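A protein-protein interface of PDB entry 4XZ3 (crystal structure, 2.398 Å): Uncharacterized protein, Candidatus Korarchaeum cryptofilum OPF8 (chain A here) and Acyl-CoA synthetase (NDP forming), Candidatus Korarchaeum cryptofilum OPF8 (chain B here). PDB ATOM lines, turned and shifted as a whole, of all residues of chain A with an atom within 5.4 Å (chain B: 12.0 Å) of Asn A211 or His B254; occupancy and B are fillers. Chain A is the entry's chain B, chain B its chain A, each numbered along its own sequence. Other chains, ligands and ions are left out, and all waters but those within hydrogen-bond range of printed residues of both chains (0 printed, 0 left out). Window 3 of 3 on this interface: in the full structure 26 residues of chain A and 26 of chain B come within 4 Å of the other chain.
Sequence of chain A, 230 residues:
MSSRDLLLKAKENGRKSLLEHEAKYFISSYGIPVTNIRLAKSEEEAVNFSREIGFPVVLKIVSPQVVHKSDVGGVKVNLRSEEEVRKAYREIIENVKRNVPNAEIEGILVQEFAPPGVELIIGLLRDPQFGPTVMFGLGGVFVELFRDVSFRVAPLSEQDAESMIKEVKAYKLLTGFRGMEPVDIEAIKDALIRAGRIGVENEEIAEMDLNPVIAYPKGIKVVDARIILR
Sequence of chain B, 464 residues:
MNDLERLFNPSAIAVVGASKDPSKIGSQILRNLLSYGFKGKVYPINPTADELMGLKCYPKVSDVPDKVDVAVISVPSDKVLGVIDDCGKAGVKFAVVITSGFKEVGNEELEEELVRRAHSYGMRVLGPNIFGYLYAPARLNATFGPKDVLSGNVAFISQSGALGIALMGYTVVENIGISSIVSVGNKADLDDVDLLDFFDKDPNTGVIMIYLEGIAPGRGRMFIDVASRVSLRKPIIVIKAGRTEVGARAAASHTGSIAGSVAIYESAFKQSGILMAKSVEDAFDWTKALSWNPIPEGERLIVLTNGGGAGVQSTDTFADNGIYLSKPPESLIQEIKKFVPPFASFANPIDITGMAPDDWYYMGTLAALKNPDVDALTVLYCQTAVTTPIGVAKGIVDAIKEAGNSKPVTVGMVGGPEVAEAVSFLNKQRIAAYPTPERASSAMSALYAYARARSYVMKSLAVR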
ATOM      1  N   LEU A 120      12.286  14.721   9.793  1.00  0.00           N
ATOM      2  CA  LEU A 120      12.049  14.833  11.231  1.00  0.00           C
ATOM      3  C   LEU A 120      10.575  14.609  11.537  1.00  0.00           C
ATOM      4  O   LEU A 120       9.737  14.681  10.642  1.00  0.00           O
ATOM      5  CB  LEU A 120      12.491  16.207  11.746  1.00  0.00           C
ATOM      6  CG  LEU A 120      13.953  16.600  11.508  1.00  0.00           C
ATOM      7  CD1 LEU A 120      14.201  18.018  11.997  1.00  0.00           C
ATOM      8  CD2 LEU A 120      14.909  15.630  12.180  1.00  0.00           C
ATOM      9  N   ILE A 121      10.262  14.325  12.797  1.00  0.00           N
ATOM     10  CA  ILE A 121       8.871  14.248  13.228  1.00  0.00           C
ATOM     11  C   ILE A 121       8.635  15.232  14.367  1.00  0.00           C
ATOM     12  O   ILE A 121       9.474  15.396  15.257  1.00  0.00           O
ATOM     13  CB  ILE A 121       8.467  12.816  13.673  1.00  0.00           C
ATOM     14  CG1 ILE A 121       6.971  12.774  13.999  1.00  0.00           C
ATOM     15  CG2 ILE A 121       9.301  12.347  14.860  1.00  0.00           C
ATOM     16  CD1 ILE A 121       6.438  11.396  14.294  1.00  0.00           C
ATOM     17  N   ILE A 122       7.487  15.898  14.301  1.00  0.00           N
ATOM     18  CA  ILE A 122       7.034  16.784  15.361  1.00  0.00           C
ATOM     19  C   ILE A 122       5.627  16.360  15.739  1.00  0.00           C
ATOM     20  O   ILE A 122       4.705  16.437  14.927  1.00  0.00           O
ATOM     21  CB  ILE A 122       7.056  18.261  14.939  1.00  0.00           C
ATOM     22  CG1 ILE A 122       8.502  18.708  14.710  1.00  0.00           C
ATOM     23  CG2 ILE A 122       6.378  19.133  16.001  1.00  0.00           C
ATOM     24  CD1 ILE A 122       8.641  20.118  14.189  1.00  0.00           C
ATOM     25  N   MET A 135       6.383  16.403  20.955  1.00  0.00           N
ATOM     26  CA  MET A 135       7.353  15.352  20.675  1.00  0.00           C
ATOM     27  C   MET A 135       8.239  15.754  19.501  1.00  0.00           C
ATOM     28  O   MET A 135       7.765  16.378  18.553  1.00  0.00           O
ATOM     29  CB  MET A 135       6.636  14.039  20.369  1.00  0.00           C
ATOM     30  CG  MET A 135       7.565  12.862  20.137  1.00  0.00           C
ATOM     31  SD  MET A 135       6.576  11.249  19.688  1.00  0.00           S
ATOM     32  CE  MET A 135       6.735  11.298  17.745  1.00  0.00           C
ATOM     33  N   GLY A 139      12.058  11.602  11.911  1.00  0.00           N
ATOM     34  CA  GLY A 139      10.798  11.225  11.313  1.00  0.00           C
ATOM     35  C   GLY A 139      11.013  10.246  10.180  1.00  0.00           C
ATOM     36  O   GLY A 139      11.852   9.351  10.259  1.00  0.00           O
ATOM     37  N   GLY A 140      10.247  10.426   9.113  1.00  0.00           N
ATOM     38  CA  GLY A 140      10.338   9.553   7.964  1.00  0.00           C
ATOM     39  C   GLY A 140       9.513   8.305   8.164  1.00  0.00           C
ATOM     40  O   GLY A 140       8.508   8.317   8.874  1.00  0.00           O
ATOM     41  N   VAL A 143      10.463   6.024  11.922  1.00  0.00           N
ATOM     42  CA  VAL A 143      10.215   6.730  13.177  1.00  0.00           C
ATOM     43  C   VAL A 143      10.140   5.732  14.321  1.00  0.00           C
ATOM     44  O   VAL A 143      10.861   5.833  15.311  1.00  0.00           O
ATOM     45  CB  VAL A 143       8.888   7.526  13.156  1.00  0.00           C
ATOM     46  CG1 VAL A 143       8.842   8.507  14.314  1.00  0.00           C
ATOM     47  CG2 VAL A 143       8.707   8.255  11.844  1.00  0.00           C
ATOM     48  N   GLU A 144       9.219   4.787  14.157  1.00  0.00           N
ATOM     49  CA  GLU A 144       8.943   3.814  15.206  1.00  0.00           C
ATOM     50  C   GLU A 144      10.094   2.832  15.414  1.00  0.00           C
ATOM     51  O   GLU A 144      10.258   2.298  16.511  1.00  0.00           O
ATOM     52  CB  GLU A 144       7.658   3.051  14.894  1.00  0.00           C
ATOM     53  CG  GLU A 144       6.445   3.967  14.711  1.00  0.00           C
ATOM     54  CD  GLU A 144       5.157   3.414  15.304  1.00  0.00           C
ATOM     55  OE1 GLU A 144       5.205   2.422  16.060  1.00  0.00           O
ATOM     56  OE2 GLU A 144       4.084   3.986  15.015  1.00  0.00           O
ATOM     57  N   ASP A 209       0.305  14.647  14.198  1.00  0.00           N
ATOM     58  CA  ASP A 209       1.503  14.101  13.581  1.00  0.00           C
ATOM     59  C   ASP A 209       1.975  14.978  12.438  1.00  0.00           C
ATOM     60  O   ASP A 209       1.327  15.043  11.399  1.00  0.00           O
ATOM     61  CB  ASP A 209       1.234  12.690  13.053  1.00  0.00           C
ATOM     62  CG  ASP A 209       1.678  11.604  14.003  1.00  0.00           C
ATOM     63  OD1 ASP A 209       1.847  11.878  15.209  1.00  0.00           O
ATOM     64  OD2 ASP A 209       1.841  10.460  13.531  1.00  0.00           O
ATOM     65  N   LEU A 210       3.093  15.663  12.637  1.00  0.00           N
ATOM     66  CA  LEU A 210       3.772  16.331  11.535  1.00  0.00           C
ATOM     67  C   LEU A 210       4.872  15.387  11.086  1.00  0.00           C
ATOM     68  O   LEU A 210       5.945  15.348  11.681  1.00  0.00           O
ATOM     69  CB  LEU A 210       4.334  17.687  11.957  1.00  0.00           C
ATOM     70  CG  LEU A 210       3.341  18.613  12.665  1.00  0.00           C
ATOM     71  CD1 LEU A 210       3.944  19.993  12.851  1.00  0.00           C
ATOM     72  CD2 LEU A 210       2.031  18.698  11.911  1.00  0.00           C
ATOM     73  N   ASN A 211       4.580  14.598  10.054  1.00  0.00           N
ATOM     74  CA  ASN A 211       5.479  13.537   9.625  1.00  0.00           C
ATOM     75  C   ASN A 211       5.337  13.209   8.140  1.00  0.00           C
ATOM     76  O   ASN A 211       4.282  12.745   7.715  1.00  0.00           O
ATOM     77  CB  ASN A 211       5.220  12.275  10.442  1.00  0.00           C
ATOM     78  CG  ASN A 211       6.207  11.163  10.132  1.00  0.00           C
ATOM     79  OD1 ASN A 211       7.383  11.416   9.868  1.00  0.00           O
ATOM     80  ND2 ASN A 211       5.727   9.926  10.158  1.00  0.00           N
ATOM     81  N   PRO A 212       6.396  13.424   7.343  1.00  0.00           N
ATOM     82  CA  PRO A 212       7.719  13.945   7.703  1.00  0.00           C
ATOM     83  C   PRO A 212       7.775  15.469   7.659  1.00  0.00           C
ATOM     84  O   PRO A 212       6.938  16.104   7.015  1.00  0.00           O
ATOM     85  CB  PRO A 212       8.631  13.330   6.647  1.00  0.00           C
ATOM     86  CG  PRO A 212       7.770  13.204   5.442  1.00  0.00           C
ATOM     87  CD  PRO A 212       6.348  13.011   5.926  1.00  0.00           C
ATOM     88  N   VAL A 213       8.747  16.027   8.373  1.00  0.00           N
ATOM     89  CA  VAL A 213       9.057  17.448   8.331  1.00  0.00           C
ATOM     90  C   VAL A 213      10.476  17.595   7.804  1.00  0.00           C
ATOM     91  O   VAL A 213      11.444  17.388   8.535  1.00  0.00           O
ATOM     92  CB  VAL A 213       8.949  18.115   9.725  1.00  0.00           C
ATOM     93  CG1 VAL A 213       9.399  19.578   9.666  1.00  0.00           C
ATOM     94  CG2 VAL A 213       7.537  18.009  10.263  1.00  0.00           C
ATOM     95  N   VAL A 222       6.604  21.098   6.166  1.00  0.00           N
ATOM     96  CA  VAL A 222       5.782  19.967   6.593  1.00  0.00           C
ATOM     97  C   VAL A 222       5.238  19.257   5.361  1.00  0.00           C
ATOM     98  O   VAL A 222       4.401  19.805   4.645  1.00  0.00           O
ATOM     99  CB  VAL A 222       4.615  20.404   7.500  1.00  0.00           C
ATOM    100  CG1 VAL A 222       3.661  19.238   7.767  1.00  0.00           C
ATOM    101  CG2 VAL A 222       5.145  20.962   8.808  1.00  0.00           C
ATOM    102  N   VAL A 223       5.710  18.039   5.111  1.00  0.00           N
ATOM    103  CA  VAL A 223       5.261  17.294   3.937  1.00  0.00           C
ATOM    104  C   VAL A 223       3.883  16.679   4.145  1.00  0.00           C
ATOM    105  O   VAL A 223       3.038  16.750   3.262  1.00  0.00           O
ATOM    106  CB  VAL A 223       6.257  16.179   3.565  1.00  0.00           C
ATOM    107  CG1 VAL A 223       5.708  15.312   2.429  1.00  0.00           C
ATOM    108  CG2 VAL A 223       7.592  16.787   3.176  1.00  0.00           C
ATOM    109  N   ASP A 224       3.661  16.064   5.301  1.00  0.00           N
ATOM    110  CA  ASP A 224       2.385  15.406   5.577  1.00  0.00           C
ATOM    111  C   ASP A 224       1.988  15.592   7.039  1.00  0.00           C
ATOM    112  O   ASP A 224       2.814  15.462   7.942  1.00  0.00           O
ATOM    113  CB  ASP A 224       2.464  13.913   5.226  1.00  0.00           C
ATOM    114  CG  ASP A 224       1.095  13.263   5.078  1.00  0.00           C
ATOM    115  OD1 ASP A 224       0.081  13.891   5.453  1.00  0.00           O
ATOM    116  OD2 ASP A 224       1.032  12.114   4.586  1.00  0.00           O
ATOM    117  N   ALA A 225       0.710  15.871   7.263  1.00  0.00           N
ATOM    118  CA  ALA A 225       0.206  16.137   8.602  1.00  0.00           C
ATOM    119  C   ALA A 225      -1.018  15.279   8.913  1.00  0.00           C
ATOM    120  O   ALA A 225      -1.762  14.888   8.014  1.00  0.00           O
ATOM    121  CB  ALA A 225      -0.126  17.603   8.756  1.00  0.00           C
ATOM    122  N   ARG A 226      -1.204  14.978  10.194  1.00  0.00           N
ATOM    123  CA  ARG A 226      -2.311  14.143  10.644  1.00  0.00           C
ATOM    124  C   ARG A 226      -2.829  14.669  11.981  1.00  0.00           C
ATOM    125  O   ARG A 226      -2.096  14.691  12.966  1.00  0.00           O
ATOM    126  CB  ARG A 226      -1.857  12.689  10.765  1.00  0.00           C
ATOM    127  CG  ARG A 226      -2.981  11.667  10.780  1.00  0.00           C
ATOM    128  CD  ARG A 226      -2.442  10.259  10.997  1.00  0.00           C
ATOM    129  NE  ARG A 226      -1.325   9.950  10.108  1.00  0.00           N
ATOM    130  CZ  ARG A 226      -0.661   8.800  10.107  1.00  0.00           C
ATOM    131  NH1 ARG A 226      -1.000   7.828  10.945  1.00  0.00           N
ATOM    132  NH2 ARG A 226       0.343   8.614   9.260  1.00  0.00           N
ATOM    133  N   GLU B 245       7.169   0.766  30.640  1.00  0.00           N
ATOM    134  CA  GLU B 245       6.126   0.975  29.645  1.00  0.00           C
ATOM    135  C   GLU B 245       5.410  -0.307  29.241  1.00  0.00           C
ATOM    136  O   GLU B 245       6.009  -1.383  29.195  1.00  0.00           O
ATOM    137  CB  GLU B 245       6.721   1.636  28.400  1.00  0.00           C
ATOM    138  CG  GLU B 245       6.499   3.133  28.340  1.00  0.00           C
ATOM    139  CD  GLU B 245       5.038   3.492  28.139  1.00  0.00           C
ATOM    140  OE1 GLU B 245       4.428   4.067  29.067  1.00  0.00           O
ATOM    141  OE2 GLU B 245       4.501   3.197  27.049  1.00  0.00           O
ATOM    142  N   GLY B 247       4.133  -0.520  26.243  1.00  0.00           N
ATOM    143  CA  GLY B 247       4.705  -0.653  24.914  1.00  0.00           C
ATOM    144  C   GLY B 247       3.693  -0.919  23.813  1.00  0.00           C
ATOM    145  O   GLY B 247       2.687  -1.596  24.028  1.00  0.00           O
ATOM    146  N   ALA B 248       3.975  -0.379  22.627  1.00  0.00           N
ATOM    147  CA  ALA B 248       3.142  -0.588  21.444  1.00  0.00           C
ATOM    148  C   ALA B 248       1.684  -0.218  21.699  1.00  0.00           C
ATOM    149  O   ALA B 248       0.835  -1.091  21.876  1.00  0.00           O
ATOM    150  CB  ALA B 248       3.244  -2.034  20.979  1.00  0.00           C
ATOM    151  N   ARG B 249       1.400   1.081  21.712  1.00  0.00           N
ATOM    152  CA  ARG B 249       0.051   1.567  21.981  1.00  0.00           C
ATOM    153  C   ARG B 249      -0.872   1.350  20.782  1.00  0.00           C
ATOM    154  O   ARG B 249      -2.069   1.121  20.950  1.00  0.00           O
ATOM    155  CB  ARG B 249       0.086   3.051  22.354  1.00  0.00           C
ATOM    156  N   ALA B 250      -0.307   1.422  19.579  1.00  0.00           N
ATOM    157  CA  ALA B 250      -1.066   1.228  18.345  1.00  0.00           C
ATOM    158  C   ALA B 250      -2.242   2.197  18.250  1.00  0.00           C
ATOM    159  O   ALA B 250      -3.399   1.779  18.221  1.00  0.00           O
ATOM    160  CB  ALA B 250      -1.560  -0.210  18.248  1.00  0.00           C
ATOM    161  N   ALA B 251      -1.934   3.490  18.194  1.00  0.00           N
ATOM    162  CA  ALA B 251      -2.954   4.535  18.148  1.00  0.00           C
ATOM    163  C   ALA B 251      -3.258   4.956  16.712  1.00  0.00           C
ATOM    164  O   ALA B 251      -2.802   4.325  15.758  1.00  0.00           O
ATOM    165  CB  ALA B 251      -2.508   5.740  18.969  1.00  0.00           C
ATOM    166  N   ALA B 252      -4.031   6.030  16.569  1.00  0.00           N
ATOM    167  CA  ALA B 252      -4.395   6.548  15.256  1.00  0.00           C
ATOM    168  C   ALA B 252      -3.297   7.447  14.690  1.00  0.00           C
ATOM    169  O   ALA B 252      -3.493   8.114  13.675  1.00  0.00           O
ATOM    170  CB  ALA B 252      -5.703   7.309  15.339  1.00  0.00           C
ATOM    171  N   SER B 253      -2.142   7.458  15.349  1.00  0.00           N
ATOM    172  CA  SER B 253      -1.024   8.290  14.927  1.00  0.00           C
ATOM    173  C   SER B 253       0.283   7.760  15.508  1.00  0.00           C
ATOM    174  O   SER B 253       0.280   7.042  16.510  1.00  0.00           O
ATOM    175  CB  SER B 253      -1.242   9.737  15.367  1.00  0.00           C
ATOM    176  OG  SER B 253      -0.906   9.889  16.734  1.00  0.00           O
ATOM    177  N   HIS B 254       1.402   8.127  14.890  1.00  0.00           N
ATOM    178  CA  HIS B 254       2.711   7.707  15.379  1.00  0.00           C
ATOM    179  C   HIS B 254       2.988   8.291  16.753  1.00  0.00           C
ATOM    180  O   HIS B 254       3.561   7.626  17.611  1.00  0.00           O
ATOM    181  CB  HIS B 254       3.824   8.118  14.412  1.00  0.00           C
ATOM    182  CG  HIS B 254       3.869   7.298  13.160  1.00  0.00           C
ATOM    183  ND1 HIS B 254       4.084   5.938  13.171  1.00  0.00           N
ATOM    184  CD2 HIS B 254       3.730   7.648  11.860  1.00  0.00           C
ATOM    185  CE1 HIS B 254       4.073   5.483  11.931  1.00  0.00           C
ATOM    186  NE2 HIS B 254       3.861   6.500  11.116  1.00  0.00           N
ATOM    187  N   THR B 255       2.596   9.543  16.954  1.00  0.00           N
ATOM    188  CA  THR B 255       2.809  10.196  18.237  1.00  0.00           C
ATOM    189  C   THR B 255       2.062   9.433  19.320  1.00  0.00           C
ATOM    190  O   THR B 255       2.627   9.106  20.363  1.00  0.00           O
ATOM    191  CB  THR B 255       2.348  11.661  18.211  1.00  0.00           C
ATOM    192  OG1 THR B 255       3.039  12.354  17.165  1.00  0.00           O
ATOM    193  CG2 THR B 255       2.635  12.348  19.547  1.00  0.00           C
ATOM    194  N   GLY B 256       0.793   9.139  19.054  1.00  0.00           N
ATOM    195  CA  GLY B 256      -0.026   8.388  19.986  1.00  0.00           C
ATOM    196  C   GLY B 256       0.564   7.031  20.317  1.00  0.00           C
ATOM    197  O   GLY B 256       0.444   6.556  21.447  1.00  0.00           O
ATOM    198  N   SER B 257       1.222   6.412  19.340  1.00  0.00           N
ATOM    199  CA  SER B 257       1.681   5.033  19.488  1.00  0.00           C
ATOM    200  C   SER B 257       3.014   4.904  20.231  1.00  0.00           C
ATOM    201  O   SER B 257       3.188   3.976  21.018  1.00  0.00           O
ATOM    202  CB  SER B 257       1.795   4.371  18.112  1.00  0.00           C
ATOM    203  OG  SER B 257       3.131   3.997  17.828  1.00  0.00           O
ATOM    204  N   ILE B 258       3.949   5.819  19.989  1.00  0.00           N
ATOM    205  CA  ILE B 258       5.275   5.703  20.599  1.00  0.00           C
ATOM    206  C   ILE B 258       5.343   6.483  21.918  1.00  0.00           C
ATOM    207  O   ILE B 258       6.105   6.140  22.821  1.00  0.00           O
ATOM    208  CB  ILE B 258       6.402   6.183  19.637  1.00  0.00           C
ATOM    209  CG1 ILE B 258       6.644   7.688  19.737  1.00  0.00           C
ATOM    210  CG2 ILE B 258       6.123   5.760  18.194  1.00  0.00           C
ATOM    211  CD1 ILE B 258       7.814   8.017  20.624  1.00  0.00           C
ATOM    212  N   ALA B 259       4.534   7.528  22.050  1.00  0.00           N
ATOM    213  CA  ALA B 259       4.530   8.303  23.287  1.00  0.00           C
ATOM    214  C   ALA B 259       3.907   7.496  24.424  1.00  0.00           C
ATOM    215  O   ALA B 259       2.782   7.008  24.303  1.00  0.00           O
ATOM    216  CB  ALA B 259       3.788   9.604  23.098  1.00  0.00           C
ATOM    217  N   GLY B 260       4.652   7.354  25.517  1.00  0.00           N
ATOM    218  CA  GLY B 260       4.169   6.663  26.702  1.00  0.00           C
ATOM    219  C   GLY B 260       4.202   7.546  27.936  1.00  0.00           C
ATOM    220  O   GLY B 260       5.031   8.459  28.037  1.00  0.00           O
ATOM    221  N   SER B 261       3.301   7.265  28.876  1.00  0.00           N
ATOM    222  CA  SER B 261       3.173   8.057  30.098  1.00  0.00           C
ATOM    223  C   SER B 261       4.480   8.104  30.887  1.00  0.00           C
ATOM    224  O   SER B 261       4.800   9.106  31.526  1.00  0.00           O
ATOM    225  CB  SER B 261       2.061   7.493  30.979  1.00  0.00           C
ATOM    226  OG  SER B 261       1.846   8.320  32.107  1.00  0.00           O
ATOM    227  N   ALA B 263       7.637   8.057  29.693  1.00  0.00           N
ATOM    228  CA  ALA B 263       8.555   9.003  29.071  1.00  0.00           C
ATOM    229  C   ALA B 263       8.106  10.440  29.314  1.00  0.00           C
ATOM    230  O   ALA B 263       8.930  11.353  29.390  1.00  0.00           O
ATOM    231  CB  ALA B 263       8.673   8.725  27.578  1.00  0.00           C
ATOM    232  N   ILE B 264       6.799  10.647  29.432  1.00  0.00           N
ATOM    233  CA  ILE B 264       6.282  11.991  29.656  1.00  0.00           C
ATOM    234  C   ILE B 264       6.550  12.427  31.090  1.00  0.00           C
ATOM    235  O   ILE B 264       6.871  13.591  31.332  1.00  0.00           O
ATOM    236  CB  ILE B 264       4.776  12.080  29.343  1.00  0.00           C
ATOM    237  CG1 ILE B 264       4.562  11.941  27.831  1.00  0.00           C
ATOM    238  CG2 ILE B 264       4.197  13.411  29.833  1.00  0.00           C
ATOM    239  CD1 ILE B 264       3.113  11.955  27.390  1.00  0.00           C
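A ring nitrogen (ND1) of His B254 sits at hydrogen-bond distance from the side-chain carboxylate of Glu A144, 2.7 Å away.
N of His B254 sits at hydrogen-bond distance from OD2 of Asp A209 (2.7 Å).
The backbone NH of Thr B255 is in hydrogen-bond range of the side-chain carboxylate of Asp A209 (3.0 Å).
OG of Ser B257 sits at hydrogen-bond distance from OE2 of Glu A144, 3.0 Å away.
Asn A211 touches just one residue of chain B: His B254 (3.5 Å).
Printed residues of chain A within 4 Å of His B254: Glu A144, Asp A209 and Asn A211.
No residue of chain B comes within 4 Å of Ile A121.
No residue of chain B comes within 4 Å of Gly A140.
No residue of chain B comes within 4 Å of Val A143.
Of the printed residues of chain B, Asp A209 touches Ser B253, His B254 and Thr B255.
No residue of chain B comes within 4 Å of Pro A212.
No residue of chain B comes within 4 Å of Val A213.
No residue of chain B comes within 4 Å of Val A222.
No residue of chain B comes within 4 Å of Val A223.
No residue of chain B comes within 4 Å of Asp A224.
No residue of chain B comes within 4 Å of Ala A225.
Of the printed residues of chain A, Ala B252 touches Arg A226.
Printed residues of chain B within 4 Å of Met A135: Thr B255 and Ile B258.
Of the printed residues of chain A, Ile B258 touches Met A135 and Glu A144.
Of the printed residues of chain A, Ser B257 touches Glu A144.
Ala B263 touches none of the printed residues of chain A.
Glu B245 touches none of the printed residues of chain A.
The nearest printed residue of chain A that does not touch His B254 is Ile A121 (4.2 Å).
The nearest printed residue of chain A that does not touch Ala B252 is Asp A209 (5.8 Å).
Of the 18 printed residues of chain A, 5 touch a printed residue of chain B.
Printed residues of chain A that touch a printed residue of chain B: Met A135, Glu A144, Asp A209, Asn A211 and Arg A226.
Printed residues of chain B that touch a printed residue of chain A: Ala B252, Ser B253, His B254, Thr B255, Ser B257 and Ile B258.
Among the printed residues, no Asp or Glu carboxylate lies within 4 Å of a Lys or Arg side-chain nitrogen of the other chain.
Among the printed residues, merely in contact across the chains: Asn A211 with His B254 (3.5 Å), Met A135 with Ile B258 (3.6 Å), Arg A226 with Ala B252 (3.6 Å), Asp A209 with Ser B253 (3.7 Å), Glu A144 with Ile B258 (3.8 Å) and Met A135 with Thr B255 (3.9 Å).
N of Gly A140 lies within hydrogen-bond range of OD1 of Asn A211, 3.1 Å away.
The backbone NH (N) of Asp A209 is in hydrogen-bond range of the backbone carbonyl oxygen (O) of Arg A226 (2.7 Å).
N of Asn A211 sits at hydrogen-bond distance from O of Asp A224 (2.9 Å).
OG of Ser B253 lies within hydrogen-bond range of N of Gly B256 (3.0 Å).
The backbone NH (N) of Arg B249 sits at hydrogen-bond distance from the backbone carbonyl oxygen (O) of Ser B257.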
